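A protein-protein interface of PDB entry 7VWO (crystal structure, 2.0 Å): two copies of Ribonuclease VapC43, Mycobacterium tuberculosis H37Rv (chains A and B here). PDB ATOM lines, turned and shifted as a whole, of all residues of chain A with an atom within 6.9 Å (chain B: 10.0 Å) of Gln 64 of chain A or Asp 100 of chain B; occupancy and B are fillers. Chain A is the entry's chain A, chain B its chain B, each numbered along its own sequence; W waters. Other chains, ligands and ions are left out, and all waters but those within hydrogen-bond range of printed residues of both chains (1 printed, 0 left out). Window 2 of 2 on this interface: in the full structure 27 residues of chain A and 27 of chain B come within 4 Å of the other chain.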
ATOM      1  N   THR A  52       2.392 -12.714  24.442  1.00  0.00           N
ATOM      2  CA  THR A  52       1.640 -12.156  25.611  1.00  0.00           C
ATOM      3  C   THR A  52       2.445 -12.367  26.899  1.00  0.00           C
ATOM      4  O   THR A  52       1.938 -11.971  27.952  1.00  0.00           O
ATOM      5  CB  THR A  52       0.271 -12.852  25.730  1.00  0.00           C
ATOM      6  OG1 THR A  52       0.470 -14.227  26.056  1.00  0.00           O
ATOM      7  CG2 THR A  52      -0.567 -12.704  24.477  1.00  0.00           C
ATOM      8  N   THR A  61       2.564  -8.315  24.037  1.00  0.00           N
ATOM      9  CA  THR A  61       1.400  -8.066  23.162  1.00  0.00           C
ATOM     10  C   THR A  61       0.139  -8.386  23.982  1.00  0.00           C
ATOM     11  O   THR A  61       0.195  -9.310  24.801  1.00  0.00           O
ATOM     12  CB  THR A  61       1.507  -8.922  21.882  1.00  0.00           C
ATOM     13  OG1 THR A  61       2.692  -8.574  21.166  1.00  0.00           O
ATOM     14  CG2 THR A  61       0.286  -8.801  20.995  1.00  0.00           C
ATOM     15  N   SER A  62      -0.937  -7.624  23.795  1.00  0.00           N
ATOM     16  CA  SER A  62      -2.230  -7.934  24.463  1.00  0.00           C
ATOM     17  C   SER A  62      -2.771  -9.263  23.917  1.00  0.00           C
ATOM     18  O   SER A  62      -2.523  -9.564  22.757  1.00  0.00           O
ATOM     19  CB  SER A  62      -3.265  -6.826  24.284  1.00  0.00           C
ATOM     20  OG  SER A  62      -3.941  -6.918  23.048  1.00  0.00           O
ATOM     21  N   PRO A  63      -3.507 -10.043  24.730  1.00  0.00           N
ATOM     22  CA  PRO A  63      -4.118 -11.287  24.270  1.00  0.00           C
ATOM     23  C   PRO A  63      -5.105 -10.924  23.142  1.00  0.00           C
ATOM     24  O   PRO A  63      -5.157 -11.638  22.172  1.00  0.00           O
ATOM     25  CB  PRO A  63      -4.810 -11.859  25.517  1.00  0.00           C
ATOM     26  CG  PRO A  63      -4.127 -11.166  26.674  1.00  0.00           C
ATOM     27  CD  PRO A  63      -3.771  -9.793  26.146  1.00  0.00           C
ATOM     28  N   GLN A  64      -5.815  -9.791  23.296  1.00  0.00           N
ATOM     29  CA  GLN A  64      -6.792  -9.375  22.250  1.00  0.00           C
ATOM     30  C   GLN A  64      -6.036  -9.139  20.932  1.00  0.00           C
ATOM     31  O   GLN A  64      -6.528  -9.591  19.894  1.00  0.00           O
ATOM     32  CB  GLN A  64      -7.480  -8.054  22.617  1.00  0.00           C
ATOM     33  CG  GLN A  64      -8.287  -8.105  23.903  1.00  0.00           C
ATOM     34  CD  GLN A  64      -7.397  -8.206  25.116  1.00  0.00           C
ATOM     35  OE1 GLN A  64      -6.344  -7.586  25.194  1.00  0.00           O
ATOM     36  NE2 GLN A  64      -7.808  -9.024  26.066  1.00  0.00           N
ATOM     37  N   ASP A  65      -4.873  -8.474  20.994  1.00  0.00           N
ATOM     38  CA  ASP A  65      -4.027  -8.267  19.783  1.00  0.00           C
ATOM     39  C   ASP A  65      -3.485  -9.604  19.251  1.00  0.00           C
ATOM     40  O   ASP A  65      -3.501  -9.798  18.036  1.00  0.00           O
ATOM     41  CB  ASP A  65      -2.910  -7.251  20.047  1.00  0.00           C
ATOM     42  CG  ASP A  65      -3.457  -5.837  20.186  1.00  0.00           C
ATOM     43  OD1 ASP A  65      -4.621  -5.625  19.809  1.00  0.00           O
ATOM     44  OD2 ASP A  65      -2.723  -4.960  20.673  1.00  0.00           O
ATOM     45  N   ALA A  66      -3.040 -10.476  20.158  1.00  0.00           N
ATOM     46  CA  ALA A  66      -2.471 -11.771  19.744  1.00  0.00           C
ATOM     47  C   ALA A  66      -3.541 -12.609  19.022  1.00  0.00           C
ATOM     48  O   ALA A  66      -3.254 -13.142  17.948  1.00  0.00           O
ATOM     49  CB  ALA A  66      -1.973 -12.466  20.982  1.00  0.00           C
ATOM     50  N   TRP A  67      -4.751 -12.646  19.586  1.00  0.00           N
ATOM     51  CA  TRP A  67      -5.853 -13.434  18.966  1.00  0.00           C
ATOM     52  C   TRP A  67      -6.240 -12.847  17.598  1.00  0.00           C
ATOM     53  O   TRP A  67      -6.454 -13.628  16.679  1.00  0.00           O
ATOM     54  CB  TRP A  67      -7.039 -13.607  19.922  1.00  0.00           C
ATOM     55  CG  TRP A  67      -6.817 -14.658  20.963  1.00  0.00           C
ATOM     56  CD1 TRP A  67      -6.576 -14.462  22.291  1.00  0.00           C
ATOM     57  CD2 TRP A  67      -6.828 -16.083  20.764  1.00  0.00           C
ATOM     58  NE1 TRP A  67      -6.438 -15.662  22.930  1.00  0.00           N
ATOM     59  CE2 TRP A  67      -6.587 -16.676  22.022  1.00  0.00           C
ATOM     60  CE3 TRP A  67      -7.014 -16.913  19.654  1.00  0.00           C
ATOM     61  CZ2 TRP A  67      -6.528 -18.057  22.195  1.00  0.00           C
ATOM     62  CZ3 TRP A  67      -6.966 -18.277  19.826  1.00  0.00           C
ATOM     63  CH2 TRP A  67      -6.726 -18.839  21.081  1.00  0.00           C
ATOM     64  N   GLN A  68      -6.298 -11.510  17.502  1.00  0.00           N
ATOM     65  CA  GLN A  68      -6.665 -10.874  16.206  1.00  0.00           C
ATOM     66  C   GLN A  68      -5.604 -11.242  15.133  1.00  0.00           C
ATOM     67  O   GLN A  68      -5.996 -11.540  14.001  1.00  0.00           O
ATOM     68  CB  GLN A  68      -6.842  -9.361  16.336  1.00  0.00           C
ATOM     69  CG  GLN A  68      -7.698  -8.762  15.232  1.00  0.00           C
ATOM     70  CD  GLN A  68      -8.889  -9.627  14.897  1.00  0.00           C
ATOM     71  OE1 GLN A  68      -9.807  -9.798  15.697  1.00  0.00           O
ATOM     72  NE2 GLN A  68      -8.875 -10.193  13.702  1.00  0.00           N
ATOM     73  N   ALA A  69      -4.319 -11.243  15.512  1.00  0.00           N
ATOM     74  CA  ALA A  69      -3.241 -11.610  14.558  1.00  0.00           C
ATOM     75  C   ALA A  69      -3.418 -13.067  14.098  1.00  0.00           C
ATOM     76  O   ALA A  69      -3.303 -13.331  12.906  1.00  0.00           O
ATOM     77  CB  ALA A  69      -1.905 -11.388  15.218  1.00  0.00           C
ATOM     78  N   PHE B  92     -10.746 -24.160  23.606  1.00  0.00           N
ATOM     79  CA  PHE B  92      -9.487 -23.508  24.057  1.00  0.00           C
ATOM     80  C   PHE B  92      -9.653 -21.976  23.987  1.00  0.00           C
ATOM     81  O   PHE B  92      -9.323 -21.278  24.949  1.00  0.00           O
ATOM     82  CB  PHE B  92      -8.347 -24.008  23.172  1.00  0.00           C
ATOM     83  CG  PHE B  92      -7.117 -23.137  23.107  1.00  0.00           C
ATOM     84  CD1 PHE B  92      -6.499 -22.686  24.262  1.00  0.00           C
ATOM     85  CD2 PHE B  92      -6.561 -22.787  21.884  1.00  0.00           C
ATOM     86  CE1 PHE B  92      -5.360 -21.900  24.197  1.00  0.00           C
ATOM     87  CE2 PHE B  92      -5.429 -21.992  21.820  1.00  0.00           C
ATOM     88  CZ  PHE B  92      -4.828 -21.549  22.976  1.00  0.00           C
ATOM     89  N   ARG B  93     -10.257 -21.501  22.887  1.00  0.00           N
ATOM     90  CA  ARG B  93     -10.490 -20.043  22.709  1.00  0.00           C
ATOM     91  C   ARG B  93     -11.451 -19.523  23.800  1.00  0.00           C
ATOM     92  O   ARG B  93     -11.192 -18.456  24.344  1.00  0.00           O
ATOM     93  CB  ARG B  93     -11.065 -19.776  21.314  1.00  0.00           C
ATOM     94  CG  ARG B  93     -11.429 -18.323  21.042  1.00  0.00           C
ATOM     95  CD  ARG B  93     -10.189 -17.518  20.712  1.00  0.00           C
ATOM     96  NE  ARG B  93     -10.403 -16.206  20.119  1.00  0.00           N
ATOM     97  CZ  ARG B  93     -10.222 -15.907  18.839  1.00  0.00           C
ATOM     98  NH1 ARG B  93      -9.855 -16.840  17.977  1.00  0.00           N
ATOM     99  NH2 ARG B  93     -10.421 -14.673  18.424  1.00  0.00           N
ATOM    100  N   GLN B  94     -12.498 -20.292  24.082  1.00  0.00           N
ATOM    101  CA  GLN B  94     -13.496 -19.857  25.101  1.00  0.00           C
ATOM    102  C   GLN B  94     -12.840 -19.754  26.488  1.00  0.00           C
ATOM    103  O   GLN B  94     -13.028 -18.741  27.153  1.00  0.00           O
ATOM    104  CB  GLN B  94     -14.612 -20.896  25.178  1.00  0.00           C
ATOM    105  CG  GLN B  94     -15.723 -20.500  26.137  1.00  0.00           C
ATOM    106  CD  GLN B  94     -16.334 -19.184  25.726  1.00  0.00           C
ATOM    107  OE1 GLN B  94     -15.942 -18.121  26.194  1.00  0.00           O
ATOM    108  NE2 GLN B  94     -17.289 -19.251  24.815  1.00  0.00           N
ATOM    109  N   LEU B  95     -12.049 -20.755  26.844  1.00  0.00           N
ATOM    110  CA  LEU B  95     -11.365 -20.758  28.167  1.00  0.00           C
ATOM    111  C   LEU B  95     -10.369 -19.587  28.261  1.00  0.00           C
ATOM    112  O   LEU B  95     -10.361 -18.904  29.301  1.00  0.00           O
ATOM    113  CB  LEU B  95     -10.658 -22.104  28.325  1.00  0.00           C
ATOM    114  CG  LEU B  95     -11.560 -23.303  28.608  1.00  0.00           C
ATOM    115  CD1 LEU B  95     -10.803 -24.608  28.417  1.00  0.00           C
ATOM    116  CD2 LEU B  95     -12.140 -23.222  30.015  1.00  0.00           C
ATOM    117  N   ALA B  96      -9.596 -19.350  27.193  1.00  0.00           N
ATOM    118  CA  ALA B  96      -8.630 -18.232  27.172  1.00  0.00           C
ATOM    119  C   ALA B  96      -9.382 -16.897  27.265  1.00  0.00           C
ATOM    120  O   ALA B  96      -8.986 -16.059  28.087  1.00  0.00           O
ATOM    121  CB  ALA B  96      -7.806 -18.277  25.911  1.00  0.00           C
ATOM    122  N   SER B  97     -10.483 -16.778  26.511  1.00  0.00           N
ATOM    123  CA  SER B  97     -11.312 -15.542  26.527  1.00  0.00           C
ATOM    124  C   SER B  97     -11.887 -15.361  27.933  1.00  0.00           C
ATOM    125  O   SER B  97     -11.857 -14.240  28.441  1.00  0.00           O
ATOM    126  CB  SER B  97     -12.417 -15.599  25.495  1.00  0.00           C
ATOM    127  OG  SER B  97     -13.416 -14.633  25.777  1.00  0.00           O
ATOM    128  N   ASP B  98     -12.284 -16.461  28.561  1.00  0.00           N
ATOM    129  CA  ASP B  98     -12.984 -16.381  29.867  1.00  0.00           C
ATOM    130  C   ASP B  98     -12.061 -15.707  30.899  1.00  0.00           C
ATOM    131  O   ASP B  98     -12.572 -14.954  31.712  1.00  0.00           O
ATOM    132  CB  ASP B  98     -13.400 -17.778  30.316  1.00  0.00           C
ATOM    133  CG  ASP B  98     -14.629 -18.355  29.633  1.00  0.00           C
ATOM    134  OD1 ASP B  98     -15.305 -17.614  28.908  1.00  0.00           O
ATOM    135  OD2 ASP B  98     -14.891 -19.553  29.837  1.00  0.00           O
ATOM    136  N   VAL B  99     -10.771 -16.029  30.880  1.00  0.00           N
ATOM    137  CA  VAL B  99      -9.810 -15.473  31.886  1.00  0.00           C
ATOM    138  C   VAL B  99      -8.895 -14.366  31.325  1.00  0.00           C
ATOM    139  O   VAL B  99      -7.977 -13.971  32.062  1.00  0.00           O
ATOM    140  CB  VAL B  99      -9.013 -16.644  32.490  1.00  0.00           C
ATOM    141  CG1 VAL B  99      -9.935 -17.702  33.076  1.00  0.00           C
ATOM    142  CG2 VAL B  99      -8.070 -17.257  31.466  1.00  0.00           C
ATOM    143  N   ASP B 100      -9.093 -13.896  30.085  1.00  0.00           N
ATOM    144  CA  ASP B 100      -8.113 -12.949  29.478  1.00  0.00           C
ATOM    145  C   ASP B 100      -6.711 -13.586  29.530  1.00  0.00           C
ATOM    146  O   ASP B 100      -5.769 -12.904  29.962  1.00  0.00           O
ATOM    147  CB  ASP B 100      -8.162 -11.563  30.135  1.00  0.00           C
ATOM    148  CG  ASP B 100      -7.558 -10.494  29.243  1.00  0.00           C
ATOM    149  OD1 ASP B 100      -7.389 -10.771  28.038  1.00  0.00           O
ATOM    150  OD2 ASP B 100      -7.247  -9.405  29.759  1.00  0.00           O
ATOM    151  N   ALA B 101      -6.587 -14.849  29.125  1.00  0.00           N
ATOM    152  CA  ALA B 101      -5.323 -15.595  29.332  1.00  0.00           C
ATOM    153  C   ALA B 101      -4.111 -14.962  28.645  1.00  0.00           C
ATOM    154  O   ALA B 101      -4.226 -14.532  27.484  1.00  0.00           O
ATOM    155  CB  ALA B 101      -5.534 -16.997  28.814  1.00  0.00           C
ATOM    156  N   ASN B 102      -2.993 -14.916  29.376  1.00  0.00           N
ATOM    157  CA  ASN B 102      -1.722 -14.399  28.806  1.00  0.00           C
ATOM    158  C   ASN B 102      -0.574 -15.298  29.287  1.00  0.00           C
ATOM    159  O   ASN B 102      -0.716 -15.920  30.341  1.00  0.00           O
ATOM    160  CB  ASN B 102      -1.498 -12.923  29.127  1.00  0.00           C
ATOM    161  CG  ASN B 102      -1.344 -12.706  30.616  1.00  0.00           C
ATOM    162  OD1 ASN B 102      -0.279 -12.950  31.174  1.00  0.00           O
ATOM    163  ND2 ASN B 102      -2.414 -12.285  31.268  1.00  0.00           N
ATOM    164  N   GLY B 103       0.489 -15.389  28.499  1.00  0.00           N
ATOM    165  CA  GLY B 103       1.647 -16.230  28.871  1.00  0.00           C
ATOM    166  C   GLY B 103       1.261 -17.688  29.093  1.00  0.00           C
ATOM    167  O   GLY B 103       0.492 -18.216  28.274  1.00  0.00           O
ATOM    168  N   ASN B 104       1.645 -18.254  30.232  1.00  0.00           N
ATOM    169  CA  ASN B 104       1.409 -19.686  30.586  1.00  0.00           C
ATOM    170  C   ASN B 104      -0.095 -20.004  30.703  1.00  0.00           C
ATOM    171  O   ASN B 104      -0.434 -21.188  30.623  1.00  0.00           O
ATOM    172  CB  ASN B 104       2.219 -20.096  31.816  1.00  0.00           C
ATOM    173  CG  ASN B 104       3.704 -19.868  31.613  1.00  0.00           C
ATOM    174  OD1 ASN B 104       4.137 -19.530  30.515  1.00  0.00           O
ATOM    175  ND2 ASN B 104       4.493 -20.038  32.662  1.00  0.00           N
ATOM    176  N   ASP B 105      -0.941 -18.986  30.895  1.00  0.00           N
ATOM    177  CA  ASP B 105      -2.403 -19.201  30.999  1.00  0.00           C
ATOM    178  C   ASP B 105      -2.820 -19.882  29.681  1.00  0.00           C
ATOM    179  O   ASP B 105      -3.742 -20.686  29.708  1.00  0.00           O
ATOM    180  CB  ASP B 105      -3.203 -17.903  31.053  1.00  0.00           C
ATOM    181  CG  ASP B 105      -2.941 -17.038  32.277  1.00  0.00           C
ATOM    182  OD1 ASP B 105      -2.490 -17.589  33.301  1.00  0.00           O
ATOM    183  OD2 ASP B 105      -3.195 -15.822  32.193  1.00  0.00           O
ATOM    184  N   ILE B 106      -2.188 -19.489  28.577  1.00  0.00           N
ATOM    185  CA  ILE B 106      -2.552 -20.058  27.250  1.00  0.00           C
ATOM    186  C   ILE B 106      -2.296 -21.575  27.252  1.00  0.00           C
ATOM    187  O   ILE B 106      -3.182 -22.323  26.803  1.00  0.00           O
ATOM    188  CB  ILE B 106      -1.721 -19.357  26.166  1.00  0.00           C
ATOM    189  CG1 ILE B 106      -2.070 -17.871  26.059  1.00  0.00           C
ATOM    190  CG2 ILE B 106      -1.877 -20.069  24.828  1.00  0.00           C
ATOM    191  CD1 ILE B 106      -3.491 -17.609  25.639  1.00  0.00           C
ATOM    192  N   ALA B 109      -4.950 -23.213  29.321  1.00  0.00           N
ATOM    193  CA  ALA B 109      -6.252 -23.191  28.609  1.00  0.00           C
ATOM    194  C   ALA B 109      -6.270 -24.317  27.557  1.00  0.00           C
ATOM    195  O   ALA B 109      -7.260 -25.053  27.478  1.00  0.00           O
ATOM    196  CB  ALA B 109      -6.462 -21.827  28.018  1.00  0.00           C
ATOM    197  N   ARG B 131      -9.646 -20.780  38.337  1.00  0.00           N
ATOM    198  CA  ARG B 131      -9.955 -19.543  37.556  1.00  0.00           C
ATOM    199  C   ARG B 131     -10.835 -19.881  36.333  1.00  0.00           C
ATOM    200  O   ARG B 131     -11.535 -18.976  35.881  1.00  0.00           O
ATOM    201  CB  ARG B 131      -8.705 -18.756  37.160  1.00  0.00           C
ATOM    202  CG  ARG B 131      -7.814 -19.383  36.099  1.00  0.00           C
ATOM    203  CD  ARG B 131      -6.487 -18.661  36.238  1.00  0.00           C
ATOM    204  NE  ARG B 131      -5.465 -18.870  35.224  1.00  0.00           N
ATOM    205  CZ  ARG B 131      -4.783 -19.992  35.050  1.00  0.00           C
ATOM    206  NH1 ARG B 131      -5.032 -21.050  35.802  1.00  0.00           N
ATOM    207  NH2 ARG B 131      -3.856 -20.058  34.114  1.00  0.00           N
ATOM    208  N   PHE B 132     -10.734 -21.102  35.787  1.00  0.00           N
ATOM    209  CA  PHE B 132     -11.645 -21.429  34.657  1.00  0.00           C
ATOM    210  C   PHE B 132     -12.979 -21.912  35.234  1.00  0.00           C
ATOM    211  O   PHE B 132     -13.121 -23.101  35.513  1.00  0.00           O
ATOM    212  CB  PHE B 132     -11.008 -22.478  33.738  1.00  0.00           C
ATOM    213  CG  PHE B 132      -9.634 -22.111  33.241  1.00  0.00           C
ATOM    214  CD1 PHE B 132      -9.476 -21.258  32.163  1.00  0.00           C
ATOM    215  CD2 PHE B 132      -8.499 -22.610  33.860  1.00  0.00           C
ATOM    216  CE1 PHE B 132      -8.212 -20.917  31.713  1.00  0.00           C
ATOM    217  CE2 PHE B 132      -7.235 -22.260  33.415  1.00  0.00           C
ATOM    218  CZ  PHE B 132      -7.095 -21.417  32.340  1.00  0.00           C
HETATM  219  O   HOH W   1      -6.298 -15.146  25.898  1.00  0.00           O
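OG1 of Thr 52 of chain A sits at hydrogen-bond distance from N of Gly 103 of chain B (2.7 Å).
The side-chain amide nitrogen (NE2) of Gln 64 of chain A sits at hydrogen-bond distance from the side-chain carboxylate (OD1) of Asp 100 of chain B, 2.7 Å away.
The side-chain hydroxyl (OG) of Ser 62 of chain A sits at hydrogen-bond distance from the side-chain amide oxygen (OE1) of Gln 64 of chain A (3.3 Å).
The backbone carbonyl oxygen of Ala 96 of chain B lies within hydrogen-bond range of the backbone NH of Ala 101 of chain B, at 2.9 Å.
The backbone NH (N) of Asn 102 of chain B sits at hydrogen-bond distance from the side-chain carboxylate (OD2) of Asp 105 of chain B (3.0 Å).
Among the printed residues, merely in contact across the chains: Thr 52 of chain A with Asn 102 of chain B (3.5 Å), Pro 63 of chain A with Asp 100 of chain B (3.6 Å), Pro 63 of chain A with Ala 101 of chain B (3.4 Å), Trp 67 of chain A with Phe 92 of chain B (3.5 Å), Trp 67 of chain A with Arg 93 of chain B (3.3 Å) and Trp 67 of chain A with Ala 96 of chain B (3.9 Å).
Gln 64 of chain A touches just one residue of chain B: Asp 100.
Printed residues of chain A within 4 Å of Asp 100 of chain B: Pro 63 (3.6 Å) and Gln 64 (2.7 Å).
No residue of chain B comes within 4 Å of Ser 62 of chain A.
Asp 65 of chain A touches none of the printed residues of chain B.
No residue of chain B comes within 4 Å of Ala 66 of chain A.
Printed residues of chain A within 4 Å of Arg 93 of chain B: Trp 67 (3.3 Å).
Of the printed residues of chain A, Asn 102 of chain B touches Thr 52.
Gln 94 of chain B touches none of the printed residues of chain A.
Val 99 of chain B touches none of the printed residues of chain A.
The nearest printed residue of chain A that does not touch Arg 93 of chain B is Gln 68 of chain A (5.3 Å).
Of the 10 printed residues of chain A, 4 touch a printed residue of chain B.
Hydrophobic or aromatic side chains of chain A that line the printed part of chain B: Pro 63 and Trp 67.
Along chain A the printed residues that touch a printed residue of chain B span positions 52 to 67.
Of the 18 printed residues of chain B, 7 touch a printed residue of chain A.
No position is printed for both chains.
Water W1 lies within hydrogen-bond range of the backbone carbonyl oxygen of Ala 101 of chain B (2.7 Å) and the indole nitrogen of Trp 67 of chain A (3.0 Å).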
